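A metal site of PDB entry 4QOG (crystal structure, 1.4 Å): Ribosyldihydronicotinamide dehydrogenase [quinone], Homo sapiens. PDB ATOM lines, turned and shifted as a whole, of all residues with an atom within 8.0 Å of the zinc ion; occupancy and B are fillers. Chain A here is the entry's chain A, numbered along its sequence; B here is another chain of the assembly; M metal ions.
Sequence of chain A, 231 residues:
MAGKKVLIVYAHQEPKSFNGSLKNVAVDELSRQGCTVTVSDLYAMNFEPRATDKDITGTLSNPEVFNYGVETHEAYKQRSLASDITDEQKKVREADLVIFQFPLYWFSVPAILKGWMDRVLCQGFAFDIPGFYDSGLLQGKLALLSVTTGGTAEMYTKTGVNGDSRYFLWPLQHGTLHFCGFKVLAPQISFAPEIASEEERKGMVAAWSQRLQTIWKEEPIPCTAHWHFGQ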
ATOM      1  N   TYR A 133      25.337   3.464   6.016  1.00  0.00           N
ATOM      2  CA  TYR A 133      25.810   4.554   5.214  1.00  0.00           C
ATOM      3  C   TYR A 133      26.795   5.398   6.035  1.00  0.00           C
ATOM      4  O   TYR A 133      27.741   4.877   6.489  1.00  0.00           O
ATOM      5  CB  TYR A 133      24.665   5.335   4.517  1.00  0.00           C
ATOM      6  CG  TYR A 133      24.020   4.562   3.380  1.00  0.00           C
ATOM      7  CD1 TYR A 133      24.766   4.090   2.342  1.00  0.00           C
ATOM      8  CD2 TYR A 133      22.663   4.297   3.365  1.00  0.00           C
ATOM      9  CE1 TYR A 133      24.193   3.362   1.326  1.00  0.00           C
ATOM     10  CE2 TYR A 133      22.093   3.561   2.355  1.00  0.00           C
ATOM     11  CZ  TYR A 133      22.851   3.094   1.337  1.00  0.00           C
ATOM     12  OH  TYR A 133      22.292   2.390   0.316  1.00  0.00           O
ATOM     13  N   ASP A 134      26.551   6.710   6.189  1.00  0.00           N
ATOM     14  CA  ASP A 134      27.504   7.532   6.875  1.00  0.00           C
ATOM     15  C   ASP A 134      27.602   7.132   8.353  1.00  0.00           C
ATOM     16  O   ASP A 134      28.562   7.482   8.961  1.00  0.00           O
ATOM     17  CB  ASP A 134      27.211   9.019   6.725  1.00  0.00           C
ATOM     18  CG  ASP A 134      27.417   9.534   5.322  1.00  0.00           C
ATOM     19  OD1 ASP A 134      27.972   8.865   4.472  1.00  0.00           O
ATOM     20  OD2 ASP A 134      26.975  10.653   5.082  1.00  0.00           O
ATOM     21  N   TRP A 170      27.661   1.127  -8.827  1.00  0.00           N
ATOM     22  CA  TRP A 170      26.736   1.476  -7.839  1.00  0.00           C
ATOM     23  C   TRP A 170      26.483   0.431  -6.753  1.00  0.00           C
ATOM     24  O   TRP A 170      26.502   0.722  -5.588  1.00  0.00           O
ATOM     25  CB  TRP A 170      25.363   1.890  -8.490  1.00  0.00           C
ATOM     26  CG  TRP A 170      24.260   2.178  -7.634  1.00  0.00           C
ATOM     27  CD1 TRP A 170      23.116   1.459  -7.492  1.00  0.00           C
ATOM     28  CD2 TRP A 170      24.050   3.393  -6.876  1.00  0.00           C
ATOM     29  NE1 TRP A 170      22.310   2.032  -6.607  1.00  0.00           N
ATOM     30  CE2 TRP A 170      22.814   3.267  -6.237  1.00  0.00           C
ATOM     31  CE3 TRP A 170      24.830   4.538  -6.637  1.00  0.00           C
ATOM     32  CZ2 TRP A 170      22.287   4.269  -5.429  1.00  0.00           C
ATOM     33  CZ3 TRP A 170      24.313   5.506  -5.842  1.00  0.00           C
ATOM     34  CH2 TRP A 170      23.074   5.392  -5.269  1.00  0.00           C
ATOM     35  N   LEU A 172      28.330  -1.966  -5.693  1.00  0.00           N
ATOM     36  CA  LEU A 172      29.581  -2.143  -5.005  1.00  0.00           C
ATOM     37  C   LEU A 172      29.998  -0.999  -4.094  1.00  0.00           C
ATOM     38  O   LEU A 172      30.164  -1.113  -2.907  1.00  0.00           O
ATOM     39  CB  LEU A 172      30.670  -2.556  -5.999  1.00  0.00           C
ATOM     40  CG  LEU A 172      30.401  -3.772  -6.923  1.00  0.00           C
ATOM     41  CD1 LEU A 172      31.426  -3.922  -8.025  1.00  0.00           C
ATOM     42  CD2 LEU A 172      30.317  -5.003  -5.999  1.00  0.00           C
ATOM     43  N   GLN A 173      30.138   0.151  -4.758  1.00  0.00           N
ATOM     44  CA  GLN A 173      30.550   1.332  -4.028  1.00  0.00           C
ATOM     45  C   GLN A 173      29.515   1.867  -3.087  1.00  0.00           C
ATOM     46  O   GLN A 173      29.806   2.110  -1.917  1.00  0.00           O
ATOM     47  CB  GLN A 173      30.944   2.466  -4.984  1.00  0.00           C
ATOM     48  CG  GLN A 173      32.162   2.073  -5.787  1.00  0.00           C
ATOM     49  CD  GLN A 173      32.771   3.150  -6.705  1.00  0.00           C
ATOM     50  OE1 GLN A 173      33.969   3.176  -6.971  1.00  0.00           O
ATOM     51  NE2 GLN A 173      31.912   4.157  -7.036  1.00  0.00           N
ATOM     52  N   HIS A 174      28.278   1.936  -3.555  1.00  0.00           N
ATOM     53  CA  HIS A 174      27.245   2.499  -2.744  1.00  0.00           C
ATOM     54  C   HIS A 174      26.522   1.470  -1.870  1.00  0.00           C
ATOM     55  O   HIS A 174      26.400   1.608  -0.637  1.00  0.00           O
ATOM     56  CB  HIS A 174      26.215   3.274  -3.606  1.00  0.00           C
ATOM     57  CG  HIS A 174      25.180   3.956  -2.790  1.00  0.00           C
ATOM     58  ND1 HIS A 174      25.444   5.097  -2.058  1.00  0.00           N
ATOM     59  CD2 HIS A 174      23.894   3.645  -2.569  1.00  0.00           C
ATOM     60  CE1 HIS A 174      24.354   5.444  -1.426  1.00  0.00           C
ATOM     61  NE2 HIS A 174      23.386   4.591  -1.739  1.00  0.00           N
ATOM     62  N   GLY A 175      25.958   0.444  -2.531  1.00  0.00           N
ATOM     63  CA  GLY A 175      25.136  -0.505  -1.809  1.00  0.00           C
ATOM     64  C   GLY A 175      25.895  -1.378  -0.828  1.00  0.00           C
ATOM     65  O   GLY A 175      25.324  -1.802   0.124  1.00  0.00           O
ATOM     66  N   THR A 176      27.239  -1.458  -1.003  1.00  0.00           N
ATOM     67  CA  THR A 176      28.033  -2.306  -0.111  1.00  0.00           C
ATOM     68  C   THR A 176      28.977  -1.418   0.693  1.00  0.00           C
ATOM     69  O   THR A 176      28.888  -1.370   1.869  1.00  0.00           O
ATOM     70  CB  THR A 176      28.795  -3.363  -0.963  1.00  0.00           C
ATOM     71  OG1 THR A 176      27.851  -4.066  -1.762  1.00  0.00           O
ATOM     72  CG2 THR A 176      29.453  -4.441  -0.006  1.00  0.00           C
ATOM     73  N   LEU A 177      29.931  -0.808   0.065  1.00  0.00           N
ATOM     74  CA  LEU A 177      31.028  -0.105   0.779  1.00  0.00           C
ATOM     75  C   LEU A 177      30.513   1.140   1.549  1.00  0.00           C
ATOM     76  O   LEU A 177      30.775   1.156   2.749  1.00  0.00           O
ATOM     77  CB  LEU A 177      32.170   0.216  -0.195  1.00  0.00           C
ATOM     78  CG  LEU A 177      32.844  -0.998  -0.898  1.00  0.00           C
ATOM     79  CD1 LEU A 177      33.759  -0.586  -2.012  1.00  0.00           C
ATOM     80  CD2 LEU A 177      33.541  -1.960   0.083  1.00  0.00           C
ATOM     81  N   HIS A 178      29.841   2.045   0.848  1.00  0.00           N
ATOM     82  CA  HIS A 178      29.286   3.198   1.593  1.00  0.00           C
ATOM     83  C   HIS A 178      28.314   2.690   2.616  1.00  0.00           C
ATOM     84  O   HIS A 178      28.334   3.230   3.704  1.00  0.00           O
ATOM     85  CB  HIS A 178      28.671   4.103   0.569  1.00  0.00           C
ATOM     86  CG  HIS A 178      28.194   5.394   1.127  1.00  0.00           C
ATOM     87  ND1 HIS A 178      27.553   6.285   0.304  1.00  0.00           N
ATOM     88  CD2 HIS A 178      28.212   5.936   2.366  1.00  0.00           C
ATOM     89  CE1 HIS A 178      27.217   7.356   1.024  1.00  0.00           C
ATOM     90  NE2 HIS A 178      27.603   7.178   2.273  1.00  0.00           N
ATOM     91  N   PHE A 179      27.494   1.696   2.349  1.00  0.00           N
ATOM     92  CA  PHE A 179      26.546   1.191   3.305  1.00  0.00           C
ATOM     93  C   PHE A 179      27.232   0.858   4.565  1.00  0.00           C
ATOM     94  O   PHE A 179      26.724   1.067   5.667  1.00  0.00           O
ATOM     95  CB  PHE A 179      25.704   0.030   2.767  1.00  0.00           C
ATOM     96  CG  PHE A 179      24.630  -0.432   3.659  1.00  0.00           C
ATOM     97  CD1 PHE A 179      23.369   0.185   3.515  1.00  0.00           C
ATOM     98  CD2 PHE A 179      24.760  -1.458   4.563  1.00  0.00           C
ATOM     99  CE1 PHE A 179      22.337  -0.270   4.293  1.00  0.00           C
ATOM    100  CE2 PHE A 179      23.681  -1.905   5.330  1.00  0.00           C
ATOM    101  CZ  PHE A 179      22.466  -1.209   5.210  1.00  0.00           C
ATOM    102  N   PHE A 182      32.388   2.865   4.746  1.00  0.00           N
ATOM    103  CA  PHE A 182      33.592   3.232   4.094  1.00  0.00           C
ATOM    104  C   PHE A 182      33.457   4.573   3.344  1.00  0.00           C
ATOM    105  O   PHE A 182      32.396   4.871   2.799  1.00  0.00           O
ATOM    106  CB  PHE A 182      34.073   2.198   2.994  1.00  0.00           C
ATOM    107  CG  PHE A 182      34.591   0.875   3.479  1.00  0.00           C
ATOM    108  CD1 PHE A 182      35.881   0.802   3.848  1.00  0.00           C
ATOM    109  CD2 PHE A 182      33.786  -0.251   3.547  1.00  0.00           C
ATOM    110  CE1 PHE A 182      36.429  -0.368   4.242  1.00  0.00           C
ATOM    111  CE2 PHE A 182      34.342  -1.467   3.947  1.00  0.00           C
ATOM    112  CZ  PHE A 182      35.673  -1.490   4.272  1.00  0.00           C
ATOM    113  N   VAL A 184      34.970   5.962  -0.084  1.00  0.00           N
ATOM    114  CA  VAL A 184      35.318   5.298  -1.285  1.00  0.00           C
ATOM    115  C   VAL A 184      36.238   6.138  -2.088  1.00  0.00           C
ATOM    116  O   VAL A 184      35.877   7.268  -2.543  1.00  0.00           O
ATOM    117  CB  VAL A 184      34.008   4.925  -2.118  1.00  0.00           C
ATOM    118  CG1 VAL A 184      34.381   4.261  -3.440  1.00  0.00           C
ATOM    119  CG2 VAL A 184      33.077   4.050  -1.244  1.00  0.00           C
ATOM    120  N   ILE A 221      35.517   9.956  -3.260  1.00  0.00           N
ATOM    121  CA  ILE A 221      34.442  10.464  -4.092  1.00  0.00           C
ATOM    122  C   ILE A 221      33.217  10.745  -3.249  1.00  0.00           C
ATOM    123  O   ILE A 221      32.985  10.247  -2.129  1.00  0.00           O
ATOM    124  CB  ILE A 221      34.030   9.456  -5.158  1.00  0.00           C
ATOM    125  CG1 ILE A 221      33.311   8.241  -4.537  1.00  0.00           C
ATOM    126  CG2 ILE A 221      35.137   9.141  -6.049  1.00  0.00           C
ATOM    127  CD1 ILE A 221      32.668   7.296  -5.519  1.00  0.00           C
ATOM    128  N   PRO A 222      32.282  11.590  -3.753  1.00  0.00           N
ATOM    129  CA  PRO A 222      31.018  11.708  -3.140  1.00  0.00           C
ATOM    130  C   PRO A 222      30.128  10.561  -3.666  1.00  0.00           C
ATOM    131  O   PRO A 222      29.813  10.512  -4.812  1.00  0.00           O
ATOM    132  CB  PRO A 222      30.534  13.098  -3.645  1.00  0.00           C
ATOM    133  CG  PRO A 222      31.166  13.200  -4.971  1.00  0.00           C
ATOM    134  CD  PRO A 222      32.460  12.427  -4.953  1.00  0.00           C
ATOM    135  N   CYS A 223      29.942   9.571  -2.820  1.00  0.00           N
ATOM    136  CA  CYS A 223      29.317   8.311  -3.274  1.00  0.00           C
ATOM    137  C   CYS A 223      27.780   8.418  -3.215  1.00  0.00           C
ATOM    138  O   CYS A 223      27.102   7.960  -2.248  1.00  0.00           O
ATOM    139  CB  CYS A 223      29.769   7.183  -2.363  1.00  0.00           C
ATOM    140  SG  CYS A 223      29.188   5.527  -2.906  1.00  0.00           S
ATOM    141  N   THR A 224      27.327   9.169  -4.245  1.00  0.00           N
ATOM    142  CA  THR A 224      25.907   9.523  -4.374  1.00  0.00           C
ATOM    143  C   THR A 224      25.437   9.061  -5.713  1.00  0.00           C
ATOM    144  O   THR A 224      26.178   8.755  -6.652  1.00  0.00           O
ATOM    145  CB  THR A 224      25.781  11.071  -4.274  1.00  0.00           C
ATOM    146  OG1 THR A 224      26.448  11.655  -5.373  1.00  0.00           O
ATOM    147  CG2 THR A 224      26.330  11.519  -2.938  1.00  0.00           C
ATOM    148  N   ALA A 225      24.099   9.122  -5.857  1.00  0.00           N
ATOM    149  CA  ALA A 225      23.466   8.875  -7.147  1.00  0.00           C
ATOM    150  C   ALA A 225      23.919   9.841  -8.217  1.00  0.00           C
ATOM    151  O   ALA A 225      24.188   9.470  -9.290  1.00  0.00           O
ATOM    152  CB  ALA A 225      21.931   8.972  -7.053  1.00  0.00           C
ATOM    153  N   TRP A 227      26.890  11.250  -8.505  1.00  0.00           N
ATOM    154  CA  TRP A 227      28.190  10.885  -9.015  1.00  0.00           C
ATOM    155  C   TRP A 227      28.108   9.714  -9.958  1.00  0.00           C
ATOM    156  O   TRP A 227      28.702   9.728 -10.962  1.00  0.00           O
ATOM    157  CB  TRP A 227      29.156  10.523  -7.826  1.00  0.00           C
ATOM    158  CG  TRP A 227      30.515  10.258  -8.190  1.00  0.00           C
ATOM    159  CD1 TRP A 227      31.558  11.157  -8.244  1.00  0.00           C
ATOM    160  CD2 TRP A 227      31.096   8.991  -8.563  1.00  0.00           C
ATOM    161  NE1 TRP A 227      32.684  10.547  -8.664  1.00  0.00           N
ATOM    162  CE2 TRP A 227      32.442   9.209  -8.818  1.00  0.00           C
ATOM    163  CE3 TRP A 227      30.581   7.704  -8.752  1.00  0.00           C
ATOM    164  CZ2 TRP A 227      33.285   8.203  -9.282  1.00  0.00           C
ATOM    165  CZ3 TRP A 227      31.461   6.699  -9.190  1.00  0.00           C
ATOM    166  CH2 TRP A 227      32.768   6.961  -9.461  1.00  0.00           C
ATOM    167  N   HIS A 228      27.261   8.761  -9.644  1.00  0.00           N
ATOM    168  CA  HIS A 228      27.180   7.567 -10.502  1.00  0.00           C
ATOM    169  C   HIS A 228      26.378   7.667 -11.834  1.00  0.00           C
ATOM    170  O   HIS A 228      26.801   7.142 -12.861  1.00  0.00           O
ATOM    171  CB  HIS A 228      26.594   6.392  -9.699  1.00  0.00           C
ATOM    172  CG  HIS A 228      27.508   5.843  -8.621  1.00  0.00           C
ATOM    173  ND1 HIS A 228      27.609   6.380  -7.375  1.00  0.00           N
ATOM    174  CD2 HIS A 228      28.317   4.741  -8.642  1.00  0.00           C
ATOM    175  CE1 HIS A 228      28.459   5.664  -6.640  1.00  0.00           C
ATOM    176  NE2 HIS A 228      28.904   4.670  -7.402  1.00  0.00           N
ATOM    177  N   VAL B 161      17.474   6.740   0.086  1.00  0.00           N
ATOM    178  CA  VAL B 161      18.876   6.343   0.524  1.00  0.00           C
ATOM    179  C   VAL B 161      19.528   5.288  -0.382  1.00  0.00           C
ATOM    180  O   VAL B 161      20.752   5.323  -0.579  1.00  0.00           O
ATOM    181  CB  VAL B 161      19.025   5.882   2.009  1.00  0.00           C
ATOM    182  CG1 VAL B 161      18.663   7.051   2.940  1.00  0.00           C
ATOM    183  CG2 VAL B 161      18.213   4.643   2.327  1.00  0.00           C
HETATM  184 ZN    ZN M   1      27.276   6.013  -1.787  1.00  0.00          ZN
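The backbone carbonyl oxygen of His 174 lies within hydrogen-bond range of the backbone NH of Phe 179, 3.2 Å away.
N of His 178 sits at hydrogen-bond distance from O of Gln 173 (2.8 Å).
The backbone carbonyl oxygen of Val 161 of chain B lies within hydrogen-bond range of a ring nitrogen (NE2) of His 174.
OD1 of Asp 134 sits at hydrogen-bond distance from NE2 of His 178, 2.8 Å away.
The backbone carbonyl oxygen (O) of Gln 173 lies close to the side-chain sulfur (SG) of Cys 223 (3.6 Å).
A ring nitrogen (NE2) of His 174 is in hydrogen-bond range of the side-chain hydroxyl (OH) of Tyr 133.
The zinc ion is bound by O of Cys 223.
ND1 of His 174 binds the zinc ion (2.1 Å).
The zinc ion is bound by ND1 of His 178 (2.1 Å).
The side-chain sulfur (SG) of Cys 223 is bound to the zinc ion.
Within 4 Å of the zinc ion: His 174, His 178 and Cys 223.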
